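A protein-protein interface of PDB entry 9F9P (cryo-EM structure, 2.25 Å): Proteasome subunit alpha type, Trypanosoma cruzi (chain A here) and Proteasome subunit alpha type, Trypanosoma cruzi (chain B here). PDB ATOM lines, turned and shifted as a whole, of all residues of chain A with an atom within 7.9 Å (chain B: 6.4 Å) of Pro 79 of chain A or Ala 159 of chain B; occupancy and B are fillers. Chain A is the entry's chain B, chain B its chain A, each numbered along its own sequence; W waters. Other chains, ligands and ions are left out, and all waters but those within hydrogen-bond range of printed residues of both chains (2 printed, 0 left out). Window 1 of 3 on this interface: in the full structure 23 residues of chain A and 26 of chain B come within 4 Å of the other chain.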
ATOM      1  N   TYR A  74       0.025  24.544  18.249  1.00  0.00           N
ATOM      2  CA  TYR A  74      -0.615  25.095  19.448  1.00  0.00           C
ATOM      3  C   TYR A  74       0.437  25.511  20.469  1.00  0.00           C
ATOM      4  O   TYR A  74       1.561  25.091  20.368  1.00  0.00           O
ATOM      5  CB  TYR A  74      -1.621  24.122  20.079  1.00  0.00           C
ATOM      6  CG  TYR A  74      -0.957  23.065  20.920  1.00  0.00           C
ATOM      7  CD1 TYR A  74      -0.697  23.260  22.263  1.00  0.00           C
ATOM      8  CD2 TYR A  74      -0.503  21.889  20.354  1.00  0.00           C
ATOM      9  CE1 TYR A  74       0.030  22.327  23.018  1.00  0.00           C
ATOM     10  CE2 TYR A  74       0.221  20.954  21.086  1.00  0.00           C
ATOM     11  CZ  TYR A  74       0.502  21.168  22.426  1.00  0.00           C
ATOM     12  OH  TYR A  74       1.181  20.204  23.158  1.00  0.00           O
ATOM     13  N   GLY A  76       0.196  26.066  24.900  1.00  0.00           N
ATOM     14  CA  GLY A  76      -0.619  26.041  26.102  1.00  0.00           C
ATOM     15  C   GLY A  76      -0.750  24.615  26.608  1.00  0.00           C
ATOM     16  O   GLY A  76       0.217  23.858  26.578  1.00  0.00           O
ATOM     17  N   ILE A  77      -1.960  24.264  27.018  1.00  0.00           N
ATOM     18  CA  ILE A  77      -2.289  22.967  27.584  1.00  0.00           C
ATOM     19  C   ILE A  77      -2.594  21.960  26.477  1.00  0.00           C
ATOM     20  O   ILE A  77      -3.646  22.018  25.842  1.00  0.00           O
ATOM     21  CB  ILE A  77      -3.489  23.206  28.525  1.00  0.00           C
ATOM     22  CG1 ILE A  77      -3.072  24.018  29.745  1.00  0.00           C
ATOM     23  CG2 ILE A  77      -4.170  21.923  28.979  1.00  0.00           C
ATOM     24  CD1 ILE A  77      -4.266  24.313  30.636  1.00  0.00           C
ATOM     25  N   GLY A  78      -1.707  20.968  26.314  1.00  0.00           N
ATOM     26  CA  GLY A  78      -1.784  19.993  25.224  1.00  0.00           C
ATOM     27  C   GLY A  78      -3.082  19.183  25.233  1.00  0.00           C
ATOM     28  O   GLY A  78      -3.778  19.047  24.230  1.00  0.00           O
ATOM     29  N   PRO A  79      -3.463  18.548  26.329  1.00  0.00           N
ATOM     30  CA  PRO A  79      -4.712  17.784  26.333  1.00  0.00           C
ATOM     31  C   PRO A  79      -5.966  18.569  25.899  1.00  0.00           C
ATOM     32  O   PRO A  79      -6.880  17.963  25.349  1.00  0.00           O
ATOM     33  CB  PRO A  79      -4.778  17.279  27.787  1.00  0.00           C
ATOM     34  CG  PRO A  79      -3.305  17.194  28.168  1.00  0.00           C
ATOM     35  CD  PRO A  79      -2.705  18.451  27.573  1.00  0.00           C
ATOM     36  N   ASP A  80      -5.969  19.898  26.116  1.00  0.00           N
ATOM     37  CA  ASP A  80      -7.048  20.752  25.640  1.00  0.00           C
ATOM     38  C   ASP A  80      -6.990  20.906  24.121  1.00  0.00           C
ATOM     39  O   ASP A  80      -8.018  20.885  23.465  1.00  0.00           O
ATOM     40  CB  ASP A  80      -7.091  22.127  26.319  1.00  0.00           C
ATOM     41  CG  ASP A  80      -7.600  22.174  27.776  1.00  0.00           C
ATOM     42  OD1 ASP A  80      -7.832  21.078  28.419  1.00  0.00           O
ATOM     43  OD2 ASP A  80      -7.748  23.320  28.300  1.00  0.00           O
ATOM     44  N   CYS A  81      -5.800  20.983  23.551  1.00  0.00           N
ATOM     45  CA  CYS A  81      -5.643  21.061  22.114  1.00  0.00           C
ATOM     46  C   CYS A  81      -6.182  19.825  21.415  1.00  0.00           C
ATOM     47  O   CYS A  81      -6.740  19.960  20.343  1.00  0.00           O
ATOM     48  CB  CYS A  81      -4.177  21.274  21.770  1.00  0.00           C
ATOM     49  SG  CYS A  81      -3.779  21.231  19.995  1.00  0.00           S
ATOM     50  N   ARG A  82      -5.982  18.617  21.975  1.00  0.00           N
ATOM     51  CA  ARG A  82      -6.488  17.393  21.359  1.00  0.00           C
ATOM     52  C   ARG A  82      -7.994  17.439  21.121  1.00  0.00           C
ATOM     53  O   ARG A  82      -8.456  16.847  20.149  1.00  0.00           O
ATOM     54  CB  ARG A  82      -6.292  16.127  22.191  1.00  0.00           C
ATOM     55  CG  ARG A  82      -4.912  15.517  22.086  1.00  0.00           C
ATOM     56  CD  ARG A  82      -4.811  14.079  22.634  1.00  0.00           C
ATOM     57  NE  ARG A  82      -5.494  13.825  23.895  1.00  0.00           N
ATOM     58  CZ  ARG A  82      -4.907  13.843  25.087  1.00  0.00           C
ATOM     59  NH1 ARG A  82      -3.598  13.983  25.185  1.00  0.00           N
ATOM     60  NH2 ARG A  82      -5.648  13.744  26.173  1.00  0.00           N
ATOM     61  N   VAL A  83      -8.748  18.085  22.023  1.00  0.00           N
ATOM     62  CA  VAL A  83     -10.187  18.173  21.866  1.00  0.00           C
ATOM     63  C   VAL A  83     -10.538  19.032  20.641  1.00  0.00           C
ATOM     64  O   VAL A  83     -11.458  18.716  19.910  1.00  0.00           O
ATOM     65  CB  VAL A  83     -10.874  18.719  23.138  1.00  0.00           C
ATOM     66  CG1 VAL A  83     -12.375  18.951  22.956  1.00  0.00           C
ATOM     67  CG2 VAL A  83     -10.650  17.840  24.347  1.00  0.00           C
ATOM     68  N   LEU A  84      -9.779  20.102  20.391  1.00  0.00           N
ATOM     69  CA  LEU A  84     -10.025  20.964  19.237  1.00  0.00           C
ATOM     70  C   LEU A  84      -9.581  20.322  17.941  1.00  0.00           C
ATOM     71  O   LEU A  84     -10.263  20.437  16.941  1.00  0.00           O
ATOM     72  CB  LEU A  84      -9.318  22.293  19.433  1.00  0.00           C
ATOM     73  CG  LEU A  84      -9.738  23.059  20.692  1.00  0.00           C
ATOM     74  CD1 LEU A  84      -8.771  24.187  20.923  1.00  0.00           C
ATOM     75  CD2 LEU A  84     -11.163  23.604  20.603  1.00  0.00           C
ATOM     76  N   VAL A  85      -8.458  19.630  17.963  1.00  0.00           N
ATOM     77  CA  VAL A  85      -8.020  18.873  16.805  1.00  0.00           C
ATOM     78  C   VAL A  85      -9.031  17.782  16.426  1.00  0.00           C
ATOM     79  O   VAL A  85      -9.292  17.631  15.235  1.00  0.00           O
ATOM     80  CB  VAL A  85      -6.611  18.299  17.033  1.00  0.00           C
ATOM     81  CG1 VAL A  85      -6.238  17.284  15.967  1.00  0.00           C
ATOM     82  CG2 VAL A  85      -5.564  19.399  17.082  1.00  0.00           C
ATOM     83  N   ARG A 126     -14.939  25.114  32.225  1.00  0.00           N
ATOM     84  CA  ARG A 126     -13.995  26.212  32.146  1.00  0.00           C
ATOM     85  C   ARG A 126     -13.533  26.378  30.699  1.00  0.00           C
ATOM     86  O   ARG A 126     -13.645  25.472  29.878  1.00  0.00           O
ATOM     87  CB  ARG A 126     -12.759  25.944  33.018  1.00  0.00           C
ATOM     88  CG  ARG A 126     -11.949  24.715  32.589  1.00  0.00           C
ATOM     89  CD  ARG A 126     -10.510  24.673  33.028  1.00  0.00           C
ATOM     90  NE  ARG A 126      -9.846  23.413  32.687  1.00  0.00           N
ATOM     91  CZ  ARG A 126      -9.327  23.122  31.501  1.00  0.00           C
ATOM     92  NH1 ARG A 126      -8.885  21.913  31.260  1.00  0.00           N
ATOM     93  NH2 ARG A 126      -9.280  24.006  30.526  1.00  0.00           N
ATOM     94  N   PHE A 128     -10.979  26.697  27.274  1.00  0.00           N
ATOM     95  CA  PHE A 128      -9.787  26.002  26.809  1.00  0.00           C
ATOM     96  C   PHE A 128      -8.550  26.832  27.117  1.00  0.00           C
ATOM     97  O   PHE A 128      -8.595  28.018  26.998  1.00  0.00           O
ATOM     98  CB  PHE A 128      -9.821  25.725  25.300  1.00  0.00           C
ATOM     99  CG  PHE A 128     -10.892  24.758  24.865  1.00  0.00           C
ATOM    100  CD1 PHE A 128     -10.710  23.396  24.971  1.00  0.00           C
ATOM    101  CD2 PHE A 128     -12.097  25.206  24.402  1.00  0.00           C
ATOM    102  CE1 PHE A 128     -11.695  22.497  24.584  1.00  0.00           C
ATOM    103  CE2 PHE A 128     -13.070  24.319  23.974  1.00  0.00           C
ATOM    104  CZ  PHE A 128     -12.889  22.958  24.117  1.00  0.00           C
ATOM    105  N   CYS A 130      -5.486  26.991  25.482  1.00  0.00           N
ATOM    106  CA  CYS A 130      -4.524  26.938  24.398  1.00  0.00           C
ATOM    107  C   CYS A 130      -4.935  27.864  23.273  1.00  0.00           C
ATOM    108  O   CYS A 130      -6.116  28.068  23.064  1.00  0.00           O
ATOM    109  CB  CYS A 130      -4.384  25.522  23.877  1.00  0.00           C
ATOM    110  SG  CYS A 130      -5.939  24.836  23.256  1.00  0.00           S
ATOM    111  N   VAL B  22      -5.569  19.398  39.648  1.00  0.00           N
ATOM    112  CA  VAL B  22      -4.674  18.520  38.897  1.00  0.00           C
ATOM    113  C   VAL B  22      -3.358  18.346  39.635  1.00  0.00           C
ATOM    114  O   VAL B  22      -2.913  17.220  39.785  1.00  0.00           O
ATOM    115  CB  VAL B  22      -4.453  19.007  37.453  1.00  0.00           C
ATOM    116  CG1 VAL B  22      -3.290  18.321  36.767  1.00  0.00           C
ATOM    117  CG2 VAL B  22      -5.706  18.861  36.605  1.00  0.00           C
ATOM    118  N   PHE B  26      -1.803  14.665  41.547  1.00  0.00           N
ATOM    119  CA  PHE B  26      -0.474  14.073  41.388  1.00  0.00           C
ATOM    120  C   PHE B  26       0.193  13.735  42.720  1.00  0.00           C
ATOM    121  O   PHE B  26       1.079  12.911  42.730  1.00  0.00           O
ATOM    122  CB  PHE B  26       0.517  15.007  40.681  1.00  0.00           C
ATOM    123  CG  PHE B  26       0.577  14.899  39.182  1.00  0.00           C
ATOM    124  CD1 PHE B  26       1.350  13.906  38.569  1.00  0.00           C
ATOM    125  CD2 PHE B  26      -0.117  15.790  38.374  1.00  0.00           C
ATOM    126  CE1 PHE B  26       1.436  13.824  37.182  1.00  0.00           C
ATOM    127  CE2 PHE B  26      -0.031  15.711  36.983  1.00  0.00           C
ATOM    128  CZ  PHE B  26       0.736  14.728  36.385  1.00  0.00           C
ATOM    129  N   ALA B 116      -6.461   8.757  27.914  1.00  0.00           N
ATOM    130  CA  ALA B 116      -6.043  10.122  28.172  1.00  0.00           C
ATOM    131  C   ALA B 116      -7.173  11.136  27.949  1.00  0.00           C
ATOM    132  O   ALA B 116      -7.240  12.107  28.668  1.00  0.00           O
ATOM    133  CB  ALA B 116      -4.816  10.450  27.360  1.00  0.00           C
ATOM    134  N   ASP B 117      -8.059  10.899  26.992  1.00  0.00           N
ATOM    135  CA  ASP B 117      -9.220  11.746  26.772  1.00  0.00           C
ATOM    136  C   ASP B 117     -10.273  11.639  27.862  1.00  0.00           C
ATOM    137  O   ASP B 117     -10.935  12.640  28.107  1.00  0.00           O
ATOM    138  CB  ASP B 117     -10.063  11.354  25.564  1.00  0.00           C
ATOM    139  CG  ASP B 117      -9.418  11.593  24.223  1.00  0.00           C
ATOM    140  OD1 ASP B 117      -8.364  12.334  24.184  1.00  0.00           O
ATOM    141  OD2 ASP B 117      -9.960  11.004  23.203  1.00  0.00           O
ATOM    142  N   ALA B 119      -9.540  11.283  30.921  1.00  0.00           N
ATOM    143  CA  ALA B 119      -9.008  12.101  31.995  1.00  0.00           C
ATOM    144  C   ALA B 119      -9.198  13.581  31.727  1.00  0.00           C
ATOM    145  O   ALA B 119      -9.432  14.324  32.637  1.00  0.00           O
ATOM    146  CB  ALA B 119      -7.539  11.826  32.172  1.00  0.00           C
ATOM    147  N   GLN B 120      -8.948  14.029  30.504  1.00  0.00           N
ATOM    148  CA  GLN B 120      -9.051  15.440  30.185  1.00  0.00           C
ATOM    149  C   GLN B 120     -10.470  15.944  30.385  1.00  0.00           C
ATOM    150  O   GLN B 120     -10.648  17.071  30.802  1.00  0.00           O
ATOM    151  CB  GLN B 120      -8.610  15.642  28.746  1.00  0.00           C
ATOM    152  CG  GLN B 120      -8.532  17.100  28.313  1.00  0.00           C
ATOM    153  CD  GLN B 120      -9.867  17.689  27.951  1.00  0.00           C
ATOM    154  OE1 GLN B 120     -10.821  17.006  27.595  1.00  0.00           O
ATOM    155  NE2 GLN B 120      -9.942  18.997  28.085  1.00  0.00           N
ATOM    156  N   THR B 123     -10.875  17.279  33.847  1.00  0.00           N
ATOM    157  CA  THR B 123     -10.207  18.500  34.213  1.00  0.00           C
ATOM    158  C   THR B 123     -10.973  19.724  33.736  1.00  0.00           C
ATOM    159  O   THR B 123     -10.618  20.838  34.073  1.00  0.00           O
ATOM    160  CB  THR B 123      -8.813  18.594  33.600  1.00  0.00           C
ATOM    161  OG1 THR B 123      -8.859  18.618  32.162  1.00  0.00           O
ATOM    162  CG2 THR B 123      -7.968  17.438  34.082  1.00  0.00           C
ATOM    163  N   LEU B 130     -11.067  13.936  39.901  1.00  0.00           N
ATOM    164  CA  LEU B 130     -10.022  13.343  39.089  1.00  0.00           C
ATOM    165  C   LEU B 130      -9.549  12.019  39.692  1.00  0.00           C
ATOM    166  O   LEU B 130      -9.519  11.861  40.916  1.00  0.00           O
ATOM    167  CB  LEU B 130      -8.827  14.282  39.063  1.00  0.00           C
ATOM    168  CG  LEU B 130      -9.110  15.710  38.667  1.00  0.00           C
ATOM    169  CD1 LEU B 130      -7.858  16.415  38.245  1.00  0.00           C
ATOM    170  CD2 LEU B 130     -10.101  15.736  37.535  1.00  0.00           C
ATOM    171  N   ASP B 157      -1.232  10.305  32.599  1.00  0.00           N
ATOM    172  CA  ASP B 157      -1.242  10.932  33.922  1.00  0.00           C
ATOM    173  C   ASP B 157      -2.600  11.562  34.215  1.00  0.00           C
ATOM    174  O   ASP B 157      -3.467  11.551  33.362  1.00  0.00           O
ATOM    175  CB  ASP B 157      -0.026  11.824  34.083  1.00  0.00           C
ATOM    176  CG  ASP B 157      -0.073  13.108  33.285  1.00  0.00           C
ATOM    177  OD1 ASP B 157       1.057  13.686  33.091  1.00  0.00           O
ATOM    178  OD2 ASP B 157      -1.215  13.610  32.971  1.00  0.00           O
ATOM    179  N   PRO B 158      -2.870  12.101  35.411  1.00  0.00           N
ATOM    180  CA  PRO B 158      -4.160  12.756  35.701  1.00  0.00           C
ATOM    181  C   PRO B 158      -4.566  14.029  34.940  1.00  0.00           C
ATOM    182  O   PRO B 158      -5.735  14.406  34.910  1.00  0.00           O
ATOM    183  CB  PRO B 158      -4.013  13.135  37.184  1.00  0.00           C
ATOM    184  CG  PRO B 158      -3.003  12.146  37.734  1.00  0.00           C
ATOM    185  CD  PRO B 158      -2.012  12.028  36.600  1.00  0.00           C
ATOM    186  N   ALA B 159      -3.614  14.735  34.352  1.00  0.00           N
ATOM    187  CA  ALA B 159      -3.929  15.889  33.512  1.00  0.00           C
ATOM    188  C   ALA B 159      -4.427  15.475  32.126  1.00  0.00           C
ATOM    189  O   ALA B 159      -4.917  16.298  31.383  1.00  0.00           O
ATOM    190  CB  ALA B 159      -2.685  16.715  33.335  1.00  0.00           C
ATOM    191  N   GLY B 160      -4.251  14.224  31.710  1.00  0.00           N
ATOM    192  CA  GLY B 160      -4.657  13.858  30.364  1.00  0.00           C
ATOM    193  C   GLY B 160      -3.491  13.839  29.385  1.00  0.00           C
ATOM    194  O   GLY B 160      -3.695  13.748  28.193  1.00  0.00           O
ATOM    195  N   TRP B 161      -2.278  13.943  29.905  1.00  0.00           N
ATOM    196  CA  TRP B 161      -1.090  13.848  29.095  1.00  0.00           C
ATOM    197  C   TRP B 161      -0.802  12.380  28.812  1.00  0.00           C
ATOM    198  O   TRP B 161      -0.968  11.540  29.670  1.00  0.00           O
ATOM    199  CB  TRP B 161       0.069  14.535  29.814  1.00  0.00           C
ATOM    200  CG  TRP B 161       1.311  14.578  28.993  1.00  0.00           C
ATOM    201  CD1 TRP B 161       1.622  15.475  28.009  1.00  0.00           C
ATOM    202  CD2 TRP B 161       2.381  13.612  29.016  1.00  0.00           C
ATOM    203  NE1 TRP B 161       2.829  15.149  27.441  1.00  0.00           N
ATOM    204  CE2 TRP B 161       3.319  14.017  28.039  1.00  0.00           C
ATOM    205  CE3 TRP B 161       2.635  12.454  29.769  1.00  0.00           C
ATOM    206  CZ2 TRP B 161       4.491  13.302  27.801  1.00  0.00           C
ATOM    207  CZ3 TRP B 161       3.797  11.751  29.539  1.00  0.00           C
ATOM    208  CH2 TRP B 161       4.711  12.175  28.567  1.00  0.00           C
ATOM    209  N   CYS B 162      -0.311  12.092  27.615  1.00  0.00           N
ATOM    210  CA  CYS B 162      -0.072  10.755  27.127  1.00  0.00           C
ATOM    211  C   CYS B 162       1.266  10.730  26.387  1.00  0.00           C
ATOM    212  O   CYS B 162       1.508  11.541  25.550  1.00  0.00           O
ATOM    213  CB  CYS B 162      -1.189  10.453  26.146  1.00  0.00           C
ATOM    214  SG  CYS B 162      -1.054   8.819  25.427  1.00  0.00           S
HETATM  215  O   HOH W   1      -6.725  19.345  30.502  1.00  0.00           O
HETATM  216  O   HOH W   2      -8.271  15.018  25.150  1.00  0.00           O
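CG of Gln 120 of chain B touches O of Pro 79 of chain A (3.5 Å).
Ala 159 of chain B touches Pro 79 of chain A (O to CG, 3.7 Å).
Pro 79 of chain A touches Gly 160 of chain B.
N of Trp 161 of chain B touches CG of Pro 79 of chain A (3.8 Å).
OE1 of Gln 120 of chain B touches CG2 of Val 83 of chain A, at 3.4 Å.
The guanidinium group (NH2) of Arg 126 of chain A lies within salt-bridge range of the side-chain carboxylate (OD2) of Asp 80 of chain A, at 2.8 Å.
The backbone NH of Trp 161 of chain B lies within hydrogen-bond range of the side-chain carboxylate of Asp 157 of chain B, 3.3 Å away.
The side-chain hydroxyl (OG1) of Thr 123 of chain B lies within hydrogen-bond range of the backbone carbonyl oxygen (O) of Gln 120 of chain B, 2.7 Å away.
The side-chain carboxylate (OD2) of Asp 157 of chain B lies within hydrogen-bond range of the backbone NH (N) of Ala 159 of chain B, 3.0 Å away.
N of Gly 160 of chain B is in hydrogen-bond range of OD2 of Asp 157 of chain B (3.3 Å).
Hydrophobic or aromatic side chains of chain B within 4 Å of the printed part of chain A: Ala 116.
Along chain B the printed residues that touch a printed residue of chain A span positions 116 to 161.
Of the 14 printed residues of chain A, 5 touch a printed residue of chain B.
Printed residues of chain A that touch a printed residue of chain B: Pro 79, Asp 80, Arg 82, Val 83 and Arg 126.
Among the printed residues, 10 pairs touch across the chains.
Water W1 lies within hydrogen-bond range of OG1 of Thr 123 of chain B (2.8 Å), OD1 of Asp 80 of chain A (2.9 Å) and NH1 of Arg 126 of chain A (3.4 Å).
Water W2 lies within hydrogen-bond range of the side-chain carboxylate of Asp 117 of chain B (2.9 Å), the guanidinium group of Arg 82 of chain A (3.1 Å) and the backbone carbonyl oxygen of Pro 79 of chain A (3.3 Å).
The guanidinium group (NE) of Arg 82 of chain A lies within salt-bridge range of the side-chain carboxylate (OD1) of Asp 117 of chain B, 3.2 Å away.
O of Gly 160 of chain B lies within hydrogen-bond range of NH2 of Arg 82 of chain A, at 2.8 Å.
O of Thr 123 of chain B sits at hydrogen-bond distance from NE of Arg 126 of chain A (3.0 Å).
The side-chain carboxylate (OD1) of Asp 80 of chain A is in hydrogen-bond range of the side-chain amide nitrogen (NE2) of Gln 120 of chain B (3.0 Å).
The backbone carbonyl oxygen (O) of Ala 116 of chain B sits at hydrogen-bond distance from the guanidinium group (NH2) of Arg 82 of chain A, at 3.4 Å.
Of chain B, only Gln 120, Ala 159, Gly 160 and Trp 161 come within 4 Å of Pro 79 of chain A.
Of chain A, only Pro 79 (3.7 Å) comes within 4 Å of Ala 159 of chain B.
Of chain A, only Pro 79 (3.5 Å) and Arg 82 (2.8 Å) come within 4 Å of Gly 160 of chain B.
Of the printed residues of chain B, Arg 82 of chain A touches Ala 116, Asp 117 and Gly 160.
Of the printed residues of chain B, Asp 80 of chain A touches Gln 120.
Gly 78 of chain A touches none of the printed residues of chain B.
The nearest residue of chain B that does not touch Pro 79 of chain A is Ala 116 of chain B (5.8 Å).
The nearest printed residue of chain A that does not touch Thr 123 of chain B is Asp 80 of chain A (4.6 Å).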
